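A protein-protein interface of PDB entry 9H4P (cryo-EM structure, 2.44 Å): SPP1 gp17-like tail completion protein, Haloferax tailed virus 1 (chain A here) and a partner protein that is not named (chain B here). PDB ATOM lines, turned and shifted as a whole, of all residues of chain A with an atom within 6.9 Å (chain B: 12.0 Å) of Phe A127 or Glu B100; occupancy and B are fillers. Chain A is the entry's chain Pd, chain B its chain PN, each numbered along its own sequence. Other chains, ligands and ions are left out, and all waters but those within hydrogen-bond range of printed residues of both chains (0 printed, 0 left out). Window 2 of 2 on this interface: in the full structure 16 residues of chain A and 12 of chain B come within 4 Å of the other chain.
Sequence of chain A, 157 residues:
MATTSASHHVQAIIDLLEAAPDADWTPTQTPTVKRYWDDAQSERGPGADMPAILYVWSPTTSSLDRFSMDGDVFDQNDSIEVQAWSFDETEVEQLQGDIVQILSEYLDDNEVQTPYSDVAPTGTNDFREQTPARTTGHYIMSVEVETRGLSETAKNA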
ATOM      1  N   TYR A  36     -25.876   4.716 -11.364  1.00  0.00           N
ATOM      2  CA  TYR A  36     -26.488   6.035 -11.254  1.00  0.00           C
ATOM      3  C   TYR A  36     -27.276   6.405 -12.516  1.00  0.00           C
ATOM      4  O   TYR A  36     -28.328   7.036 -12.412  1.00  0.00           O
ATOM      5  CB  TYR A  36     -25.417   7.065 -10.898  1.00  0.00           C
ATOM      6  CG  TYR A  36     -25.859   8.498 -10.746  1.00  0.00           C
ATOM      7  CD1 TYR A  36     -25.971   9.338 -11.847  1.00  0.00           C
ATOM      8  CD2 TYR A  36     -26.066   9.045  -9.488  1.00  0.00           C
ATOM      9  CE1 TYR A  36     -26.313  10.675 -11.705  1.00  0.00           C
ATOM     10  CE2 TYR A  36     -26.408  10.379  -9.328  1.00  0.00           C
ATOM     11  CZ  TYR A  36     -26.525  11.198 -10.439  1.00  0.00           C
ATOM     12  OH  TYR A  36     -26.877  12.505 -10.262  1.00  0.00           O
ATOM     13  N   TRP A  57     -21.711   4.682  -8.626  1.00  0.00           N
ATOM     14  CA  TRP A  57     -20.891   5.200  -9.717  1.00  0.00           C
ATOM     15  C   TRP A  57     -19.474   5.506  -9.218  1.00  0.00           C
ATOM     16  O   TRP A  57     -19.223   5.462  -8.015  1.00  0.00           O
ATOM     17  CB  TRP A  57     -21.566   6.415 -10.381  1.00  0.00           C
ATOM     18  CG  TRP A  57     -21.362   7.716  -9.660  1.00  0.00           C
ATOM     19  CD1 TRP A  57     -20.488   8.702 -10.013  1.00  0.00           C
ATOM     20  CD2 TRP A  57     -22.027   8.182  -8.463  1.00  0.00           C
ATOM     21  NE1 TRP A  57     -20.560   9.743  -9.127  1.00  0.00           N
ATOM     22  CE2 TRP A  57     -21.494   9.457  -8.163  1.00  0.00           C
ATOM     23  CE3 TRP A  57     -23.015   7.661  -7.612  1.00  0.00           C
ATOM     24  CZ2 TRP A  57     -21.918  10.206  -7.059  1.00  0.00           C
ATOM     25  CZ3 TRP A  57     -23.433   8.401  -6.522  1.00  0.00           C
ATOM     26  CH2 TRP A  57     -22.891   9.659  -6.249  1.00  0.00           C
ATOM     27  N   GLU A  81     -18.728   6.021  -5.153  1.00  0.00           N
ATOM     28  CA  GLU A  81     -19.722   6.459  -4.186  1.00  0.00           C
ATOM     29  C   GLU A  81     -21.012   5.656  -4.368  1.00  0.00           C
ATOM     30  O   GLU A  81     -21.433   5.394  -5.496  1.00  0.00           O
ATOM     31  CB  GLU A  81     -19.945   7.969  -4.290  1.00  0.00           C
ATOM     32  CG  GLU A  81     -20.921   8.516  -3.262  1.00  0.00           C
ATOM     33  CD  GLU A  81     -20.886  10.020  -3.060  1.00  0.00           C
ATOM     34  OE1 GLU A  81     -20.143  10.701  -3.785  1.00  0.00           O
ATOM     35  OE2 GLU A  81     -21.605  10.510  -2.180  1.00  0.00           O
ATOM     36  N   GLN A  83     -24.941   6.062  -3.171  1.00  0.00           N
ATOM     37  CA  GLN A  83     -25.975   6.905  -2.578  1.00  0.00           C
ATOM     38  C   GLN A  83     -27.222   6.073  -2.272  1.00  0.00           C
ATOM     39  O   GLN A  83     -27.714   5.361  -3.144  1.00  0.00           O
ATOM     40  CB  GLN A  83     -26.376   8.037  -3.531  1.00  0.00           C
ATOM     41  CG  GLN A  83     -25.530   9.302  -3.433  1.00  0.00           C
ATOM     42  CD  GLN A  83     -26.078  10.445  -4.259  1.00  0.00           C
ATOM     43  OE1 GLN A  83     -27.041  10.306  -5.012  1.00  0.00           O
ATOM     44  NE2 GLN A  83     -25.456  11.604  -4.125  1.00  0.00           N
ATOM     45  N   TRP A  85     -31.239   6.324  -1.326  1.00  0.00           N
ATOM     46  CA  TRP A  85     -32.388   7.221  -1.448  1.00  0.00           C
ATOM     47  C   TRP A  85     -33.637   6.567  -0.844  1.00  0.00           C
ATOM     48  O   TRP A  85     -33.955   5.429  -1.193  1.00  0.00           O
ATOM     49  CB  TRP A  85     -32.654   7.594  -2.922  1.00  0.00           C
ATOM     50  CG  TRP A  85     -31.666   8.469  -3.645  1.00  0.00           C
ATOM     51  CD1 TRP A  85     -30.316   8.284  -3.756  1.00  0.00           C
ATOM     52  CD2 TRP A  85     -31.966   9.626  -4.458  1.00  0.00           C
ATOM     53  NE1 TRP A  85     -29.760   9.261  -4.541  1.00  0.00           N
ATOM     54  CE2 TRP A  85     -30.747  10.098  -4.996  1.00  0.00           C
ATOM     55  CE3 TRP A  85     -33.141  10.325  -4.781  1.00  0.00           C
ATOM     56  CZ2 TRP A  85     -30.680  11.230  -5.819  1.00  0.00           C
ATOM     57  CZ3 TRP A  85     -33.076  11.438  -5.598  1.00  0.00           C
ATOM     58  CH2 TRP A  85     -31.857  11.889  -6.110  1.00  0.00           C
ATOM     59  N   GLN A  96     -27.071   3.396   5.264  1.00  0.00           N
ATOM     60  CA  GLN A  96     -25.679   3.813   5.384  1.00  0.00           C
ATOM     61  C   GLN A  96     -24.893   2.840   6.267  1.00  0.00           C
ATOM     62  O   GLN A  96     -23.785   2.446   5.904  1.00  0.00           O
ATOM     63  CB  GLN A  96     -25.578   5.255   5.885  1.00  0.00           C
ATOM     64  CG  GLN A  96     -24.155   5.681   6.223  1.00  0.00           C
ATOM     65  CD  GLN A  96     -24.029   7.176   6.372  1.00  0.00           C
ATOM     66  OE1 GLN A  96     -24.050   7.709   7.479  1.00  0.00           O
ATOM     67  NE2 GLN A  96     -23.892   7.869   5.252  1.00  0.00           N
ATOM     68  N   THR A 124     -18.158   8.482   4.818  1.00  0.00           N
ATOM     69  CA  THR A 124     -19.606   8.492   4.661  1.00  0.00           C
ATOM     70  C   THR A 124     -20.127   9.926   4.738  1.00  0.00           C
ATOM     71  O   THR A 124     -19.572  10.748   5.465  1.00  0.00           O
ATOM     72  CB  THR A 124     -20.302   7.626   5.722  1.00  0.00           C
ATOM     73  OG1 THR A 124     -20.010   8.141   7.022  1.00  0.00           O
ATOM     74  CG2 THR A 124     -19.923   6.160   5.684  1.00  0.00           C
ATOM     75  N   ASN A 125     -21.209  10.204   3.997  1.00  0.00           N
ATOM     76  CA  ASN A 125     -21.826  11.521   3.981  1.00  0.00           C
ATOM     77  C   ASN A 125     -23.289  11.413   4.401  1.00  0.00           C
ATOM     78  O   ASN A 125     -23.973  10.443   4.073  1.00  0.00           O
ATOM     79  CB  ASN A 125     -21.720  12.192   2.607  1.00  0.00           C
ATOM     80  CG  ASN A 125     -20.299  12.309   2.097  1.00  0.00           C
ATOM     81  OD1 ASN A 125     -19.512  13.101   2.605  1.00  0.00           O
ATOM     82  ND2 ASN A 125     -19.966  11.531   1.080  1.00  0.00           N
ATOM     83  N   ASP A 126     -23.739  12.433   5.137  1.00  0.00           N
ATOM     84  CA  ASP A 126     -25.140  12.684   5.423  1.00  0.00           C
ATOM     85  C   ASP A 126     -25.557  13.914   4.615  1.00  0.00           C
ATOM     86  O   ASP A 126     -24.838  14.913   4.616  1.00  0.00           O
ATOM     87  CB  ASP A 126     -25.311  12.882   6.934  1.00  0.00           C
ATOM     88  CG  ASP A 126     -26.743  13.014   7.426  1.00  0.00           C
ATOM     89  OD1 ASP A 126     -27.665  13.042   6.589  1.00  0.00           O
ATOM     90  OD2 ASP A 126     -26.922  13.089   8.657  1.00  0.00           O
ATOM     91  N   PHE A 127     -26.705  13.838   3.922  1.00  0.00           N
ATOM     92  CA  PHE A 127     -27.246  14.985   3.202  1.00  0.00           C
ATOM     93  C   PHE A 127     -28.695  15.265   3.607  1.00  0.00           C
ATOM     94  O   PHE A 127     -29.405  15.930   2.855  1.00  0.00           O
ATOM     95  CB  PHE A 127     -27.130  14.818   1.678  1.00  0.00           C
ATOM     96  CG  PHE A 127     -25.748  14.525   1.153  1.00  0.00           C
ATOM     97  CD1 PHE A 127     -24.710  15.435   1.323  1.00  0.00           C
ATOM     98  CD2 PHE A 127     -25.484  13.340   0.479  1.00  0.00           C
ATOM     99  CE1 PHE A 127     -23.438  15.160   0.842  1.00  0.00           C
ATOM    100  CE2 PHE A 127     -24.214  13.069  -0.007  1.00  0.00           C
ATOM    101  CZ  PHE A 127     -23.195  13.983   0.169  1.00  0.00           C
ATOM    102  N   ARG A 128     -29.126  14.782   4.786  1.00  0.00           N
ATOM    103  CA  ARG A 128     -30.512  14.909   5.226  1.00  0.00           C
ATOM    104  C   ARG A 128     -30.886  16.372   5.476  1.00  0.00           C
ATOM    105  O   ARG A 128     -32.065  16.717   5.376  1.00  0.00           O
ATOM    106  CB  ARG A 128     -30.788  14.043   6.459  1.00  0.00           C
ATOM    107  CG  ARG A 128     -30.874  12.553   6.152  1.00  0.00           C
ATOM    108  CD  ARG A 128     -30.995  11.669   7.381  1.00  0.00           C
ATOM    109  NE  ARG A 128     -29.828  11.785   8.251  1.00  0.00           N
ATOM    110  CZ  ARG A 128     -29.629  11.119   9.386  1.00  0.00           C
ATOM    111  NH1 ARG A 128     -28.523  11.327  10.082  1.00  0.00           N
ATOM    112  NH2 ARG A 128     -30.522  10.249   9.827  1.00  0.00           N
ATOM    113  N   GLU A 129     -29.881  17.219   5.766  1.00  0.00           N
ATOM    114  CA  GLU A 129     -30.057  18.655   5.969  1.00  0.00           C
ATOM    115  C   GLU A 129     -30.572  19.365   4.710  1.00  0.00           C
ATOM    116  O   GLU A 129     -31.062  20.490   4.808  1.00  0.00           O
ATOM    117  CB  GLU A 129     -28.777  19.294   6.524  1.00  0.00           C
ATOM    118  CG  GLU A 129     -27.645  19.437   5.515  1.00  0.00           C
ATOM    119  CD  GLU A 129     -26.778  18.218   5.249  1.00  0.00           C
ATOM    120  OE1 GLU A 129     -27.103  17.130   5.758  1.00  0.00           O
ATOM    121  OE2 GLU A 129     -25.773  18.365   4.535  1.00  0.00           O
ATOM    122  N   GLN A 130     -30.481  18.708   3.542  1.00  0.00           N
ATOM    123  CA  GLN A 130     -30.824  19.304   2.255  1.00  0.00           C
ATOM    124  C   GLN A 130     -32.311  19.168   1.916  1.00  0.00           C
ATOM    125  O   GLN A 130     -32.834  20.004   1.180  1.00  0.00           O
ATOM    126  CB  GLN A 130     -29.964  18.700   1.143  1.00  0.00           C
ATOM    127  CG  GLN A 130     -28.472  18.913   1.361  1.00  0.00           C
ATOM    128  CD  GLN A 130     -27.679  18.857   0.080  1.00  0.00           C
ATOM    129  OE1 GLN A 130     -27.972  18.082  -0.828  1.00  0.00           O
ATOM    130  NE2 GLN A 130     -26.648  19.682  -0.003  1.00  0.00           N
ATOM    131  N   THR A 131     -32.974  18.120   2.432  1.00  0.00           N
ATOM    132  CA  THR A 131     -34.345  17.770   2.073  1.00  0.00           C
ATOM    133  C   THR A 131     -35.318  18.830   2.598  1.00  0.00           C
ATOM    134  O   THR A 131     -35.414  19.002   3.816  1.00  0.00           O
ATOM    135  CB  THR A 131     -34.704  16.372   2.603  1.00  0.00           C
ATOM    136  OG1 THR A 131     -33.727  15.442   2.133  1.00  0.00           O
ATOM    137  CG2 THR A 131     -36.081  15.900   2.189  1.00  0.00           C
ATOM    138  N   HIS A 138     -36.937  12.848  -1.174  1.00  0.00           N
ATOM    139  CA  HIS A 138     -35.973  11.869  -0.699  1.00  0.00           C
ATOM    140  C   HIS A 138     -34.987  12.487   0.283  1.00  0.00           C
ATOM    141  O   HIS A 138     -34.465  13.577   0.054  1.00  0.00           O
ATOM    142  CB  HIS A 138     -35.251  11.213  -1.879  1.00  0.00           C
ATOM    143  CG  HIS A 138     -36.217  10.580  -2.813  1.00  0.00           C
ATOM    144  ND1 HIS A 138     -36.717  11.232  -3.922  1.00  0.00           N
ATOM    145  CD2 HIS A 138     -36.833   9.383  -2.762  1.00  0.00           C
ATOM    146  CE1 HIS A 138     -37.576  10.447  -4.537  1.00  0.00           C
ATOM    147  NE2 HIS A 138     -37.661   9.309  -3.845  1.00  0.00           N
ATOM    148  N   TYR A 139     -34.752  11.752   1.373  1.00  0.00           N
ATOM    149  CA  TYR A 139     -33.535  11.872   2.156  1.00  0.00           C
ATOM    150  C   TYR A 139     -32.429  11.111   1.431  1.00  0.00           C
ATOM    151  O   TYR A 139     -32.690  10.065   0.836  1.00  0.00           O
ATOM    152  CB  TYR A 139     -33.775  11.359   3.579  1.00  0.00           C
ATOM    153  CG  TYR A 139     -34.778  12.201   4.324  1.00  0.00           C
ATOM    154  CD1 TYR A 139     -34.404  13.426   4.858  1.00  0.00           C
ATOM    155  CD2 TYR A 139     -36.109  11.818   4.438  1.00  0.00           C
ATOM    156  CE1 TYR A 139     -35.316  14.238   5.510  1.00  0.00           C
ATOM    157  CE2 TYR A 139     -37.035  12.619   5.089  1.00  0.00           C
ATOM    158  CZ  TYR A 139     -36.636  13.832   5.627  1.00  0.00           C
ATOM    159  OH  TYR A 139     -37.536  14.625   6.277  1.00  0.00           O
ATOM    160  N   ILE A 140     -31.204  11.653   1.473  1.00  0.00           N
ATOM    161  CA  ILE A 140     -30.057  11.047   0.808  1.00  0.00           C
ATOM    162  C   ILE A 140     -28.901  10.957   1.802  1.00  0.00           C
ATOM    163  O   ILE A 140     -28.650  11.900   2.549  1.00  0.00           O
ATOM    164  CB  ILE A 140     -29.659  11.817  -0.478  1.00  0.00           C
ATOM    165  CG1 ILE A 140     -30.834  12.029  -1.440  1.00  0.00           C
ATOM    166  CG2 ILE A 140     -28.480  11.148  -1.183  1.00  0.00           C
ATOM    167  CD1 ILE A 140     -30.602  13.102  -2.489  1.00  0.00           C
ATOM    168  N   MET A 141     -28.222   9.802   1.800  1.00  0.00           N
ATOM    169  CA  MET A 141     -26.965   9.585   2.503  1.00  0.00           C
ATOM    170  C   MET A 141     -26.062   8.746   1.597  1.00  0.00           C
ATOM    171  O   MET A 141     -26.564   8.090   0.684  1.00  0.00           O
ATOM    172  CB  MET A 141     -27.199   8.860   3.835  1.00  0.00           C
ATOM    173  CG  MET A 141     -28.093   9.624   4.808  1.00  0.00           C
ATOM    174  SD  MET A 141     -28.326   8.809   6.402  1.00  0.00           S
ATOM    175  CE  MET A 141     -26.867   9.365   7.280  1.00  0.00           C
ATOM    176  N   SER A 142     -24.740   8.764   1.837  1.00  0.00           N
ATOM    177  CA  SER A 142     -23.831   8.044   0.955  1.00  0.00           C
ATOM    178  C   SER A 142     -22.648   7.411   1.689  1.00  0.00           C
ATOM    179  O   SER A 142     -22.300   7.810   2.801  1.00  0.00           O
ATOM    180  CB  SER A 142     -23.382   8.907  -0.207  1.00  0.00           C
ATOM    181  OG  SER A 142     -22.381   9.833   0.192  1.00  0.00           O
ATOM    182  N   GLU A 144     -18.615   6.501   0.661  1.00  0.00           N
ATOM    183  CA  GLU A 144     -17.469   6.566  -0.230  1.00  0.00           C
ATOM    184  C   GLU A 144     -16.638   5.303  -0.033  1.00  0.00           C
ATOM    185  O   GLU A 144     -16.360   4.915   1.102  1.00  0.00           O
ATOM    186  CB  GLU A 144     -16.640   7.820   0.047  1.00  0.00           C
ATOM    187  CG  GLU A 144     -17.394   9.111  -0.217  1.00  0.00           C
ATOM    188  CD  GLU A 144     -16.619  10.387   0.033  1.00  0.00           C
ATOM    189  OE1 GLU A 144     -15.379  10.358  -0.050  1.00  0.00           O
ATOM    190  OE2 GLU A 144     -17.262  11.412   0.307  1.00  0.00           O
ATOM    191  N   SER B  96     -38.907  23.754  -9.165  1.00  0.00           N
ATOM    192  CA  SER B  96     -37.544  23.249  -9.264  1.00  0.00           C
ATOM    193  C   SER B  96     -37.067  22.704  -7.915  1.00  0.00           C
ATOM    194  O   SER B  96     -37.485  23.193  -6.868  1.00  0.00           O
ATOM    195  CB  SER B  96     -36.607  24.312  -9.798  1.00  0.00           C
ATOM    196  OG  SER B  96     -35.277  23.825  -9.904  1.00  0.00           O
ATOM    197  N   GLU B  97     -36.188  21.688  -7.964  1.00  0.00           N
ATOM    198  CA  GLU B  97     -35.542  21.075  -6.806  1.00  0.00           C
ATOM    199  C   GLU B  97     -34.051  20.888  -7.108  1.00  0.00           C
ATOM    200  O   GLU B  97     -33.695  20.609  -8.251  1.00  0.00           O
ATOM    201  CB  GLU B  97     -36.166  19.710  -6.493  1.00  0.00           C
ATOM    202  CG  GLU B  97     -37.648  19.736  -6.155  1.00  0.00           C
ATOM    203  CD  GLU B  97     -38.276  18.363  -6.010  1.00  0.00           C
ATOM    204  OE1 GLU B  97     -38.249  17.597  -6.986  1.00  0.00           O
ATOM    205  OE2 GLU B  97     -38.780  18.063  -4.916  1.00  0.00           O
ATOM    206  N   SER B  98     -33.189  21.022  -6.082  1.00  0.00           N
ATOM    207  CA  SER B  98     -31.739  20.914  -6.231  1.00  0.00           C
ATOM    208  C   SER B  98     -31.072  20.432  -4.936  1.00  0.00           C
ATOM    209  O   SER B  98     -31.541  20.750  -3.846  1.00  0.00           O
ATOM    210  CB  SER B  98     -31.149  22.229  -6.695  1.00  0.00           C
ATOM    211  OG  SER B  98     -29.758  22.109  -6.957  1.00  0.00           O
ATOM    212  N   GLY B  99     -29.961  19.683  -5.071  1.00  0.00           N
ATOM    213  CA  GLY B  99     -29.152  19.187  -3.960  1.00  0.00           C
ATOM    214  C   GLY B  99     -28.038  18.248  -4.433  1.00  0.00           C
ATOM    215  O   GLY B  99     -27.718  18.235  -5.619  1.00  0.00           O
ATOM    216  N   GLU B 100     -27.478  17.444  -3.511  1.00  0.00           N
ATOM    217  CA  GLU B 100     -26.440  16.463  -3.827  1.00  0.00           C
ATOM    218  C   GLU B 100     -26.988  15.252  -4.591  1.00  0.00           C
ATOM    219  O   GLU B 100     -26.217  14.396  -5.025  1.00  0.00           O
ATOM    220  CB  GLU B 100     -25.656  16.062  -2.575  1.00  0.00           C
ATOM    221  CG  GLU B 100     -24.752  17.156  -2.037  1.00  0.00           C
ATOM    222  CD  GLU B 100     -23.622  17.606  -2.947  1.00  0.00           C
ATOM    223  OE1 GLU B 100     -23.150  16.796  -3.759  1.00  0.00           O
ATOM    224  OE2 GLU B 100     -23.220  18.771  -2.837  1.00  0.00           O
ATOM    225  N   GLY B 101     -28.313  15.187  -4.765  1.00  0.00           N
ATOM    226  CA  GLY B 101     -28.937  14.267  -5.704  1.00  0.00           C
ATOM    227  C   GLY B 101     -28.947  14.789  -7.144  1.00  0.00           C
ATOM    228  O   GLY B 101     -29.416  14.087  -8.039  1.00  0.00           O
ATOM    229  N   GLY B 102     -28.426  16.009  -7.363  1.00  0.00           N
ATOM    230  CA  GLY B 102     -28.554  16.725  -8.628  1.00  0.00           C
ATOM    231  C   GLY B 102     -29.776  17.649  -8.644  1.00  0.00           C
ATOM    232  O   GLY B 102     -30.365  17.896  -7.593  1.00  0.00           O
ATOM    233  N   SER B 103     -30.166  18.141  -9.838  1.00  0.00           N
ATOM    234  CA  SER B 103     -31.165  19.201  -9.983  1.00  0.00           C
ATOM    235  C   SER B 103     -32.192  18.915 -11.085  1.00  0.00           C
ATOM    236  O   SER B 103     -31.886  18.217 -12.049  1.00  0.00           O
ATOM    237  CB  SER B 103     -30.508  20.541 -10.218  1.00  0.00           C
ATOM    238  OG  SER B 103     -29.514  20.811  -9.243  1.00  0.00           O
ATOM    239  N   VAL B 104     -33.390  19.518 -10.954  1.00  0.00           N
ATOM    240  CA  VAL B 104     -34.517  19.342 -11.870  1.00  0.00           C
ATOM    241  C   VAL B 104     -35.381  20.611 -11.908  1.00  0.00           C
ATOM    242  O   VAL B 104     -35.418  21.356 -10.932  1.00  0.00           O
ATOM    243  CB  VAL B 104     -35.339  18.081 -11.508  1.00  0.00           C
ATOM    244  CG1 VAL B 104     -35.833  18.075 -10.066  1.00  0.00           C
ATOM    245  CG2 VAL B 104     -36.479  17.792 -12.479  1.00  0.00           C
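Among the printed residues, merely in contact across the chains: Tyr A36 with Gly B101, Trp A85 with Gly B101, Phe A127 with Glu B100, Gln A130 with Gly B99 and Ile A140 with Gly B101.
Of the 20 printed residues of chain A, 6 touch a printed residue of chain B.
Among the printed residues, 7 pairs touch across the chains.
Among the printed residues, no Asp or Glu carboxylate lies within 4 Å of a Lys or Arg side-chain nitrogen of the other chain.
Of the printed residues of chain B, Phe A127 touches Glu B100.
Printed residues of chain A within 4 Å of Glu B100: Gln A83, Phe A127 and Gln A130.
No residue of chain B comes within 4 Å of Asn A125.
No residue of chain B comes within 4 Å of Asp A126.
No residue of chain B comes within 4 Å of Arg A128.
No residue of chain B comes within 4 Å of Glu A129.
No residue of chain B comes within 4 Å of Thr A131.
No residue of chain B comes within 4 Å of Met A141.
No residue of chain B comes within 4 Å of Ser A142.
Printed residues of chain B within 4 Å of Tyr A36: Gly B101 (3.7 Å).
Of the printed residues of chain A, Gly B101 touches Tyr A36, Trp A85 and Ile A140.
Printed residues of chain A within 4 Å of Gly B99: Gln A130 (3.5 Å).
Gly B102 touches none of the printed residues of chain A.
The nearest residue of chain B that does not touch Phe A127 is Gly B101 (6.2 Å).
The nearest residue of chain A that does not touch Glu B100 is Ile A140 (4.7 Å).
The nearest printed residue of chain B that does not touch Trp A85 is Gly B102 (5.5 Å).
The side-chain amide oxygen (OE1) of Gln A83 sits at hydrogen-bond distance from the indole nitrogen (NE1) of Trp A85 (3.0 Å).
O of Ile A140 is in hydrogen-bond range of N of Phe A127, 3.1 Å away.
The side-chain amide nitrogen (NE2) of Gln A83 sits at hydrogen-bond distance from the backbone carbonyl oxygen (O) of Glu B100.
OE1 of Gln A130 is in hydrogen-bond range of N of Glu B100, at 2.8 Å.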
